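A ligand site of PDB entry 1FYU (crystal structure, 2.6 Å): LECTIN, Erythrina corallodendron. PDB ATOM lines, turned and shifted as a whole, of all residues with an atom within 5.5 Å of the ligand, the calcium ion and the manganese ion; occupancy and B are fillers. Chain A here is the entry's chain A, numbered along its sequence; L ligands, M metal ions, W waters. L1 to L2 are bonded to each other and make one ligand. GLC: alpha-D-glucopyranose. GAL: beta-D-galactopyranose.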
ATOM      1  N   PRO A  85     -19.300 -19.762  30.777  1.00  0.00           N
ATOM      2  CA  PRO A  85     -18.645 -19.311  29.545  1.00  0.00           C
ATOM      3  C   PRO A  85     -19.085 -17.875  29.232  1.00  0.00           C
ATOM      4  O   PRO A  85     -19.805 -17.269  30.013  1.00  0.00           O
ATOM      5  CB  PRO A  85     -19.154 -20.301  28.513  1.00  0.00           C
ATOM      6  CG  PRO A  85     -20.569 -20.562  28.989  1.00  0.00           C
ATOM      7  CD  PRO A  85     -20.375 -20.730  30.477  1.00  0.00           C
ATOM      8  N   LEU A  86     -18.635 -17.345  28.101  1.00  0.00           N
ATOM      9  CA  LEU A  86     -19.001 -15.993  27.692  1.00  0.00           C
ATOM     10  C   LEU A  86     -20.504 -15.887  27.427  1.00  0.00           C
ATOM     11  O   LEU A  86     -21.109 -16.776  26.821  1.00  0.00           O
ATOM     12  CB  LEU A  86     -18.212 -15.580  26.454  1.00  0.00           C
ATOM     13  CG  LEU A  86     -16.879 -14.869  26.715  1.00  0.00           C
ATOM     14  CD1 LEU A  86     -16.010 -15.707  27.623  1.00  0.00           C
ATOM     15  CD2 LEU A  86     -16.179 -14.608  25.406  1.00  0.00           C
ATOM     16  N   ALA A  88     -24.136 -14.677  25.773  1.00  0.00           N
ATOM     17  CA  ALA A  88     -24.604 -14.523  24.397  1.00  0.00           C
ATOM     18  C   ALA A  88     -26.138 -14.499  24.408  1.00  0.00           C
ATOM     19  O   ALA A  88     -26.739 -14.926  25.386  1.00  0.00           O
ATOM     20  CB  ALA A  88     -24.090 -15.673  23.546  1.00  0.00           C
ATOM     21  N   ASP A  89     -26.787 -14.012  23.343  1.00  0.00           N
ATOM     22  CA  ASP A  89     -26.134 -13.482  22.160  1.00  0.00           C
ATOM     23  C   ASP A  89     -26.424 -12.000  21.938  1.00  0.00           C
ATOM     24  O   ASP A  89     -25.605 -11.271  21.376  1.00  0.00           O
ATOM     25  CB  ASP A  89     -26.563 -14.290  20.927  1.00  0.00           C
ATOM     26  CG  ASP A  89     -25.614 -15.449  20.614  1.00  0.00           C
ATOM     27  OD1 ASP A  89     -25.913 -16.609  21.000  1.00  0.00           O
ATOM     28  OD2 ASP A  89     -24.566 -15.192  19.988  1.00  0.00           O
ATOM     29  N   TYR A 106     -29.145 -17.921  18.240  1.00  0.00           N
ATOM     30  CA  TYR A 106     -27.755 -17.598  18.564  1.00  0.00           C
ATOM     31  C   TYR A 106     -27.332 -16.271  17.936  1.00  0.00           C
ATOM     32  O   TYR A 106     -28.082 -15.297  17.983  1.00  0.00           O
ATOM     33  CB  TYR A 106     -26.816 -18.723  18.113  1.00  0.00           C
ATOM     34  CG  TYR A 106     -27.302 -20.098  18.507  1.00  0.00           C
ATOM     35  CD1 TYR A 106     -27.868 -20.335  19.761  1.00  0.00           C
ATOM     36  CD2 TYR A 106     -27.256 -21.160  17.596  1.00  0.00           C
ATOM     37  CE1 TYR A 106     -28.382 -21.594  20.099  1.00  0.00           C
ATOM     38  CE2 TYR A 106     -27.767 -22.423  17.921  1.00  0.00           C
ATOM     39  CZ  TYR A 106     -28.333 -22.620  19.162  1.00  0.00           C
ATOM     40  OH  TYR A 106     -28.885 -23.848  19.479  1.00  0.00           O
ATOM     41  N   GLY A 107     -26.136 -16.242  17.357  1.00  0.00           N
ATOM     42  CA  GLY A 107     -25.618 -15.032  16.750  1.00  0.00           C
ATOM     43  C   GLY A 107     -26.463 -14.433  15.636  1.00  0.00           C
ATOM     44  O   GLY A 107     -26.209 -13.313  15.197  1.00  0.00           O
ATOM     45  N   GLU A 127     -28.905  -3.731  16.209  1.00  0.00           N
ATOM     46  CA  GLU A 127     -28.602  -4.745  17.199  1.00  0.00           C
ATOM     47  C   GLU A 127     -27.772  -4.268  18.394  1.00  0.00           C
ATOM     48  O   GLU A 127     -27.080  -3.239  18.348  1.00  0.00           O
ATOM     49  CB  GLU A 127     -27.845  -5.888  16.510  1.00  0.00           C
ATOM     50  CG  GLU A 127     -26.434  -5.490  16.095  1.00  0.00           C
ATOM     51  CD  GLU A 127     -25.642  -6.618  15.466  1.00  0.00           C
ATOM     52  OE1 GLU A 127     -24.404  -6.590  15.582  1.00  0.00           O
ATOM     53  OE2 GLU A 127     -26.243  -7.516  14.833  1.00  0.00           O
ATOM     54  N   ASP A 129     -25.461  -6.438  20.240  1.00  0.00           N
ATOM     55  CA  ASP A 129     -24.731  -7.699  20.197  1.00  0.00           C
ATOM     56  C   ASP A 129     -23.792  -7.876  21.388  1.00  0.00           C
ATOM     57  O   ASP A 129     -22.937  -7.028  21.632  1.00  0.00           O
ATOM     58  CB  ASP A 129     -23.912  -7.719  18.897  1.00  0.00           C
ATOM     59  CG  ASP A 129     -23.542  -9.102  18.471  1.00  0.00           C
ATOM     60  OD1 ASP A 129     -23.397  -9.979  19.350  1.00  0.00           O
ATOM     61  OD2 ASP A 129     -23.367  -9.326  17.257  1.00  0.00           O
ATOM     62  N   THR A 130     -23.949  -8.982  22.099  1.00  0.00           N
ATOM     63  CA  THR A 130     -23.125  -9.252  23.272  1.00  0.00           C
ATOM     64  C   THR A 130     -22.095 -10.364  23.085  1.00  0.00           C
ATOM     65  O   THR A 130     -21.310 -10.641  24.007  1.00  0.00           O
ATOM     66  CB  THR A 130     -23.992  -9.587  24.489  1.00  0.00           C
ATOM     67  OG1 THR A 130     -24.747 -10.770  24.229  1.00  0.00           O
ATOM     68  CG2 THR A 130     -24.934  -8.428  24.809  1.00  0.00           C
ATOM     69  N   PHE A 131     -22.093 -11.013  21.933  1.00  0.00           N
ATOM     70  CA  PHE A 131     -21.144 -12.082  21.668  1.00  0.00           C
ATOM     71  C   PHE A 131     -20.479 -11.875  20.311  1.00  0.00           C
ATOM     72  O   PHE A 131     -21.134 -11.609  19.314  1.00  0.00           O
ATOM     73  CB  PHE A 131     -21.829 -13.442  21.713  1.00  0.00           C
ATOM     74  CG  PHE A 131     -20.897 -14.603  21.497  1.00  0.00           C
ATOM     75  CD1 PHE A 131     -20.533 -14.992  20.206  1.00  0.00           C
ATOM     76  CD2 PHE A 131     -20.339 -15.268  22.589  1.00  0.00           C
ATOM     77  CE1 PHE A 131     -19.621 -16.033  20.001  1.00  0.00           C
ATOM     78  CE2 PHE A 131     -19.425 -16.318  22.395  1.00  0.00           C
ATOM     79  CZ  PHE A 131     -19.066 -16.707  21.096  1.00  0.00           C
ATOM     80  N   SER A 132     -19.158 -12.024  20.278  1.00  0.00           N
ATOM     81  CA  SER A 132     -18.412 -11.824  19.047  1.00  0.00           C
ATOM     82  C   SER A 132     -18.273 -13.048  18.148  1.00  0.00           C
ATOM     83  O   SER A 132     -17.447 -13.930  18.398  1.00  0.00           O
ATOM     84  CB  SER A 132     -17.022 -11.291  19.381  1.00  0.00           C
ATOM     85  OG  SER A 132     -16.350 -10.956  18.187  1.00  0.00           O
ATOM     86  N   ASN A 133     -19.083 -13.092  17.091  1.00  0.00           N
ATOM     87  CA  ASN A 133     -19.040 -14.194  16.147  1.00  0.00           C
ATOM     88  C   ASN A 133     -17.951 -13.920  15.094  1.00  0.00           C
ATOM     89  O   ASN A 133     -17.291 -12.881  15.130  1.00  0.00           O
ATOM     90  CB  ASN A 133     -20.396 -14.353  15.448  1.00  0.00           C
ATOM     91  CG  ASN A 133     -21.515 -14.636  16.424  1.00  0.00           C
ATOM     92  OD1 ASN A 133     -22.034 -13.724  17.064  1.00  0.00           O
ATOM     93  ND2 ASN A 133     -21.895 -15.899  16.552  1.00  0.00           N
ATOM     94  N   TRP A 135     -18.156 -12.949  12.119  1.00  0.00           N
ATOM     95  CA  TRP A 135     -18.457 -11.745  11.354  1.00  0.00           C
ATOM     96  C   TRP A 135     -18.495 -10.467  12.183  1.00  0.00           C
ATOM     97  O   TRP A 135     -18.708  -9.388  11.650  1.00  0.00           O
ATOM     98  CB  TRP A 135     -19.801 -11.921  10.646  1.00  0.00           C
ATOM     99  CG  TRP A 135     -20.921 -12.235  11.587  1.00  0.00           C
ATOM    100  CD1 TRP A 135     -21.603 -11.346  12.375  1.00  0.00           C
ATOM    101  CD2 TRP A 135     -21.446 -13.530  11.898  1.00  0.00           C
ATOM    102  NE1 TRP A 135     -22.528 -12.003  13.153  1.00  0.00           N
ATOM    103  CE2 TRP A 135     -22.451 -13.347  12.888  1.00  0.00           C
ATOM    104  CE3 TRP A 135     -21.174 -14.827  11.454  1.00  0.00           C
ATOM    105  CZ2 TRP A 135     -23.178 -14.421  13.429  1.00  0.00           C
ATOM    106  CZ3 TRP A 135     -21.902 -15.901  11.995  1.00  0.00           C
ATOM    107  CH2 TRP A 135     -22.893 -15.682  12.975  1.00  0.00           C
ATOM    108  N   ASP A 136     -18.281 -10.591  13.489  1.00  0.00           N
ATOM    109  CA  ASP A 136     -18.313  -9.438  14.389  1.00  0.00           C
ATOM    110  C   ASP A 136     -16.956  -8.825  14.647  1.00  0.00           C
ATOM    111  O   ASP A 136     -15.928  -9.457  14.407  1.00  0.00           O
ATOM    112  CB  ASP A 136     -18.885  -9.830  15.757  1.00  0.00           C
ATOM    113  CG  ASP A 136     -20.377 -10.015  15.742  1.00  0.00           C
ATOM    114  OD1 ASP A 136     -21.070  -9.096  15.269  1.00  0.00           O
ATOM    115  OD2 ASP A 136     -20.862 -11.059  16.227  1.00  0.00           O
ATOM    116  N   PRO A 137     -16.936  -7.574  15.112  1.00  0.00           N
ATOM    117  CA  PRO A 137     -15.657  -6.928  15.424  1.00  0.00           C
ATOM    118  C   PRO A 137     -15.255  -7.600  16.741  1.00  0.00           C
ATOM    119  O   PRO A 137     -16.056  -8.329  17.328  1.00  0.00           O
ATOM    120  CB  PRO A 137     -16.047  -5.462  15.596  1.00  0.00           C
ATOM    121  CG  PRO A 137     -17.479  -5.531  16.069  1.00  0.00           C
ATOM    122  CD  PRO A 137     -18.044  -6.597  15.173  1.00  0.00           C
ATOM    123  N   HIS A 142     -21.746  -4.400  21.446  1.00  0.00           N
ATOM    124  CA  HIS A 142     -21.633  -3.323  20.476  1.00  0.00           C
ATOM    125  C   HIS A 142     -22.986  -3.075  19.829  1.00  0.00           C
ATOM    126  O   HIS A 142     -23.827  -3.973  19.745  1.00  0.00           O
ATOM    127  CB  HIS A 142     -20.588  -3.641  19.399  1.00  0.00           C
ATOM    128  CG  HIS A 142     -20.887  -4.872  18.579  1.00  0.00           C
ATOM    129  ND1 HIS A 142     -20.147  -6.032  18.686  1.00  0.00           N
ATOM    130  CD2 HIS A 142     -21.829  -5.111  17.638  1.00  0.00           C
ATOM    131  CE1 HIS A 142     -20.622  -6.930  17.847  1.00  0.00           C
ATOM    132  NE2 HIS A 142     -21.645  -6.399  17.192  1.00  0.00           N
ATOM    133  N   ILE A 150     -26.367  -9.933   9.022  1.00  0.00           N
ATOM    134  CA  ILE A 150     -25.979  -9.913  10.413  1.00  0.00           C
ATOM    135  C   ILE A 150     -24.605  -9.264  10.490  1.00  0.00           C
ATOM    136  O   ILE A 150     -24.154  -8.868  11.557  1.00  0.00           O
ATOM    137  CB  ILE A 150     -25.890 -11.337  10.998  1.00  0.00           C
ATOM    138  CG1 ILE A 150     -25.801 -11.273  12.518  1.00  0.00           C
ATOM    139  CG2 ILE A 150     -24.671 -12.059  10.426  1.00  0.00           C
ATOM    140  CD1 ILE A 150     -27.028 -10.656  13.182  1.00  0.00           C
ATOM    141  N   SER A 152     -22.939  -6.311  10.281  1.00  0.00           N
ATOM    142  CA  SER A 152     -23.227  -4.878  10.337  1.00  0.00           C
ATOM    143  C   SER A 152     -22.412  -4.017   9.389  1.00  0.00           C
ATOM    144  O   SER A 152     -21.248  -4.308   9.138  1.00  0.00           O
ATOM    145  CB  SER A 152     -23.001  -4.363  11.759  1.00  0.00           C
ATOM    146  OG  SER A 152     -23.755  -5.091  12.712  1.00  0.00           O
ATOM    147  N   THR A 155     -20.545  -0.256  13.186  1.00  0.00           N
ATOM    148  CA  THR A 155     -20.492  -0.782  14.532  1.00  0.00           C
ATOM    149  C   THR A 155     -19.995   0.225  15.572  1.00  0.00           C
ATOM    150  O   THR A 155     -19.123   1.046  15.274  1.00  0.00           O
ATOM    151  CB  THR A 155     -19.595  -2.042  14.521  1.00  0.00           C
ATOM    152  OG1 THR A 155     -20.424  -3.198  14.601  1.00  0.00           O
ATOM    153  CG2 THR A 155     -18.576  -2.016  15.631  1.00  0.00           C
ATOM    154  N   THR A 216     -30.255 -16.399  23.338  1.00  0.00           N
ATOM    155  CA  THR A 216     -29.162 -16.801  24.210  1.00  0.00           C
ATOM    156  C   THR A 216     -28.326 -17.841  23.478  1.00  0.00           C
ATOM    157  O   THR A 216     -28.769 -18.390  22.468  1.00  0.00           O
ATOM    158  CB  THR A 216     -29.673 -17.364  25.552  1.00  0.00           C
ATOM    159  OG1 THR A 216     -30.720 -18.314  25.318  1.00  0.00           O
ATOM    160  CG2 THR A 216     -30.193 -16.237  26.432  1.00  0.00           C
ATOM    161  N   GLY A 217     -27.123 -18.093  23.984  1.00  0.00           N
ATOM    162  CA  GLY A 217     -26.175 -19.005  23.355  1.00  0.00           C
ATOM    163  C   GLY A 217     -26.447 -20.467  23.075  1.00  0.00           C
ATOM    164  O   GLY A 217     -27.410 -21.072  23.576  1.00  0.00           O
ATOM    165  N   ALA A 218     -25.535 -21.046  22.285  1.00  0.00           N
ATOM    166  CA  ALA A 218     -25.615 -22.440  21.862  1.00  0.00           C
ATOM    167  C   ALA A 218     -25.049 -23.479  22.832  1.00  0.00           C
ATOM    168  O   ALA A 218     -25.146 -24.674  22.563  1.00  0.00           O
ATOM    169  CB  ALA A 218     -24.941 -22.608  20.504  1.00  0.00           C
ATOM    170  N   GLN A 219     -24.434 -23.049  23.920  1.00  0.00           N
ATOM    171  CA  GLN A 219     -23.927 -24.015  24.881  1.00  0.00           C
ATOM    172  C   GLN A 219     -24.362 -23.613  26.292  1.00  0.00           C
ATOM    173  O   GLN A 219     -24.715 -22.468  26.540  1.00  0.00           O
ATOM    174  CB  GLN A 219     -22.399 -24.122  24.792  1.00  0.00           C
ATOM    175  CG  GLN A 219     -21.651 -22.972  25.382  1.00  0.00           C
ATOM    176  CD  GLN A 219     -20.151 -23.156  25.252  1.00  0.00           C
ATOM    177  OE1 GLN A 219     -19.593 -23.016  24.162  1.00  0.00           O
ATOM    178  NE2 GLN A 219     -19.491 -23.473  26.355  1.00  0.00           N
ATOM    179  N   ALA A 222     -24.277 -20.089  28.362  1.00  0.00           N
ATOM    180  CA  ALA A 222     -23.838 -18.990  27.508  1.00  0.00           C
ATOM    181  C   ALA A 222     -25.154 -18.243  27.363  1.00  0.00           C
ATOM    182  O   ALA A 222     -25.812 -18.272  26.323  1.00  0.00           O
ATOM    183  CB  ALA A 222     -23.366 -19.499  26.159  1.00  0.00           C
HETATM  184  C1  GLC L   1     -19.601 -25.250  19.224  1.00  0.00           C
HETATM  185  C2  GLC L   1     -19.942 -24.575  20.556  1.00  0.00           C
HETATM  186  C3  GLC L   1     -21.040 -23.530  20.343  1.00  0.00           C
HETATM  187  C4  GLC L   1     -20.634 -22.537  19.247  1.00  0.00           C
HETATM  188  C5  GLC L   1     -20.181 -23.272  17.973  1.00  0.00           C
HETATM  189  C6  GLC L   1     -19.558 -22.311  16.973  1.00  0.00           C
HETATM  190  O1  GLC L   1     -20.745 -25.846  18.700  1.00  0.00           O
HETATM  191  O2  GLC L   1     -20.386 -25.554  21.484  1.00  0.00           O
HETATM  192  O3  GLC L   1     -21.261 -22.830  21.557  1.00  0.00           O
HETATM  193  O4  GLC L   1     -21.745 -21.666  18.937  1.00  0.00           O
HETATM  194  O5  GLC L   1     -19.156 -24.253  18.283  1.00  0.00           O
HETATM  195  O6  GLC L   1     -20.007 -22.595  15.663  1.00  0.00           O
HETATM  196  C1  GAL L   2     -21.629 -20.348  19.373  1.00  0.00           C
HETATM  197  C2  GAL L   2     -22.660 -19.471  18.646  1.00  0.00           C
HETATM  198  C3  GAL L   2     -22.636 -18.038  19.227  1.00  0.00           C
HETATM  199  C4  GAL L   2     -22.795 -18.070  20.747  1.00  0.00           C
HETATM  200  C5  GAL L   2     -21.742 -18.997  21.351  1.00  0.00           C
HETATM  201  C6  GAL L   2     -21.871 -19.144  22.852  1.00  0.00           C
HETATM  202  O2  GAL L   2     -22.357 -19.436  17.258  1.00  0.00           O
HETATM  203  O3  GAL L   2     -23.687 -17.277  18.660  1.00  0.00           O
HETATM  204  O4  GAL L   2     -24.094 -18.543  21.075  1.00  0.00           O
HETATM  205  O5  GAL L   2     -21.876 -20.332  20.783  1.00  0.00           O
HETATM  206  O6  GAL L   2     -20.939 -20.074  23.356  1.00  0.00           O
HETATM  207 CA    CA M   1     -22.667 -11.616  17.598  1.00  0.00          CA
HETATM  208 MN    MN M   2     -22.650  -7.860  15.717  1.00  0.00          MN
HETATM  209  O   HOH W   1     -19.150 -18.386  17.058  1.00  0.00           O
HETATM  210  O   HOH W   2     -24.303 -12.719  18.910  1.00  0.00           O
HETATM  211  O   HOH W   3     -22.014  -6.730  14.030  1.00  0.00           O
HETATM  212  O   HOH W   4     -19.812 -18.903  25.621  1.00  0.00           O
HETATM  213  O   HOH W   5     -24.344 -11.591  15.798  1.00  0.00           O
HETATM  214  O   HOH W   6     -24.058  -9.140  14.500  1.00  0.00           O
HETATM  215  O   HOH W   7     -18.460 -20.441  21.904  1.00  0.00           O
HETATM  216  O   HOH W   8     -21.381 -21.887  12.527  1.00  0.00           O
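OE1 of Glu 127 lies close to OG of Ser 152 (3.3 Å).
The side-chain carboxylate (OD2) of Asp 89 sits at hydrogen-bond distance from the backbone NH (N) of Gly 107, 3.2 Å away.
The backbone carbonyl oxygen (O) of Asp 89 lies within hydrogen-bond range of the backbone NH (N) of Thr 130, at 2.9 Å.
The backbone NH (N) of Gly 217 lies within hydrogen-bond range of the backbone carbonyl oxygen (O) of Ala 222 (2.7 Å).
The backbone NH (N) of Gly 217 is in hydrogen-bond range of the backbone carbonyl oxygen (O) of Ala 88 (3.5 Å).
Within 4 Å of the calcium ion: Asp 129, Phe 131, Asn 133 and Asp 136.
The nearest printed residue that does not touch the manganese ion is Ser 152 (4.2 Å).
Merely in contact with the ligand: Gly 217 (3.1 Å), Tyr 106 (3.5 Å), Ala 222 (3.6 Å) and Ala 88 (3.8 Å).
The nearest printed residue that does not touch the ligand is Leu 86 (4.7 Å).
An oxygen (O3) of GAL L2 is in hydrogen-bond range of the side-chain amide nitrogen of Asn 133 (3.1 Å).
An oxygen (O3) of GAL L2 lies within hydrogen-bond range of the side-chain carboxylate of Asp 89 (2.6 Å).
N of Gly 107 is in hydrogen-bond range of O3 of GAL L2 (3.0 Å).
An oxygen (O3) of GLC L1 sits at hydrogen-bond distance from the side-chain amide oxygen of Gln 219 (3.1 Å).
The backbone NH of Ala 218 sits at hydrogen-bond distance from an oxygen (O4) of GAL L2 (3.1 Å).
The calcium ion is bound by the side-chain amide oxygen (OD1) of Asn 133 (2.3 Å), the backbone carbonyl oxygen (O) of Phe 131 (2.3 Å), the side-chain carboxylate (OD2) of Asp 136 (2.3 Å), water W2 (2.4 Å), the side-chain carboxylate (OD2) of Asp 129 (2.4 Å), water W5 (2.5 Å) and the side-chain carboxylate (OD1) of Asp 129 (2.5 Å).
The calcium ion has seven donor atoms within binding distance.
Water W5 lies within hydrogen-bond range of O of Gly 107 (2.6 Å) and NE1 of Trp 135 (3.2 Å).
Water W6 lies within hydrogen-bond range of the side-chain carboxylate of Glu 127 and the backbone carbonyl oxygen of Ile 150.
Water W4 bridges O of Leu 86 and O6 of GAL L2.
The manganese ion is bound by OD1 of Asp 136 (2.1 Å).
The manganese ion is bound by water W3 (2.1 Å).
OE1 of Glu 127 is bound to the manganese ion.
The manganese ion is bound by OD2 of Asp 129, at 2.2 Å.
Water W6 binds the manganese ion (2.3 Å).
NE2 of His 142 binds the manganese ion, 2.3 Å away.
The manganese ion has six donor atoms within binding distance.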
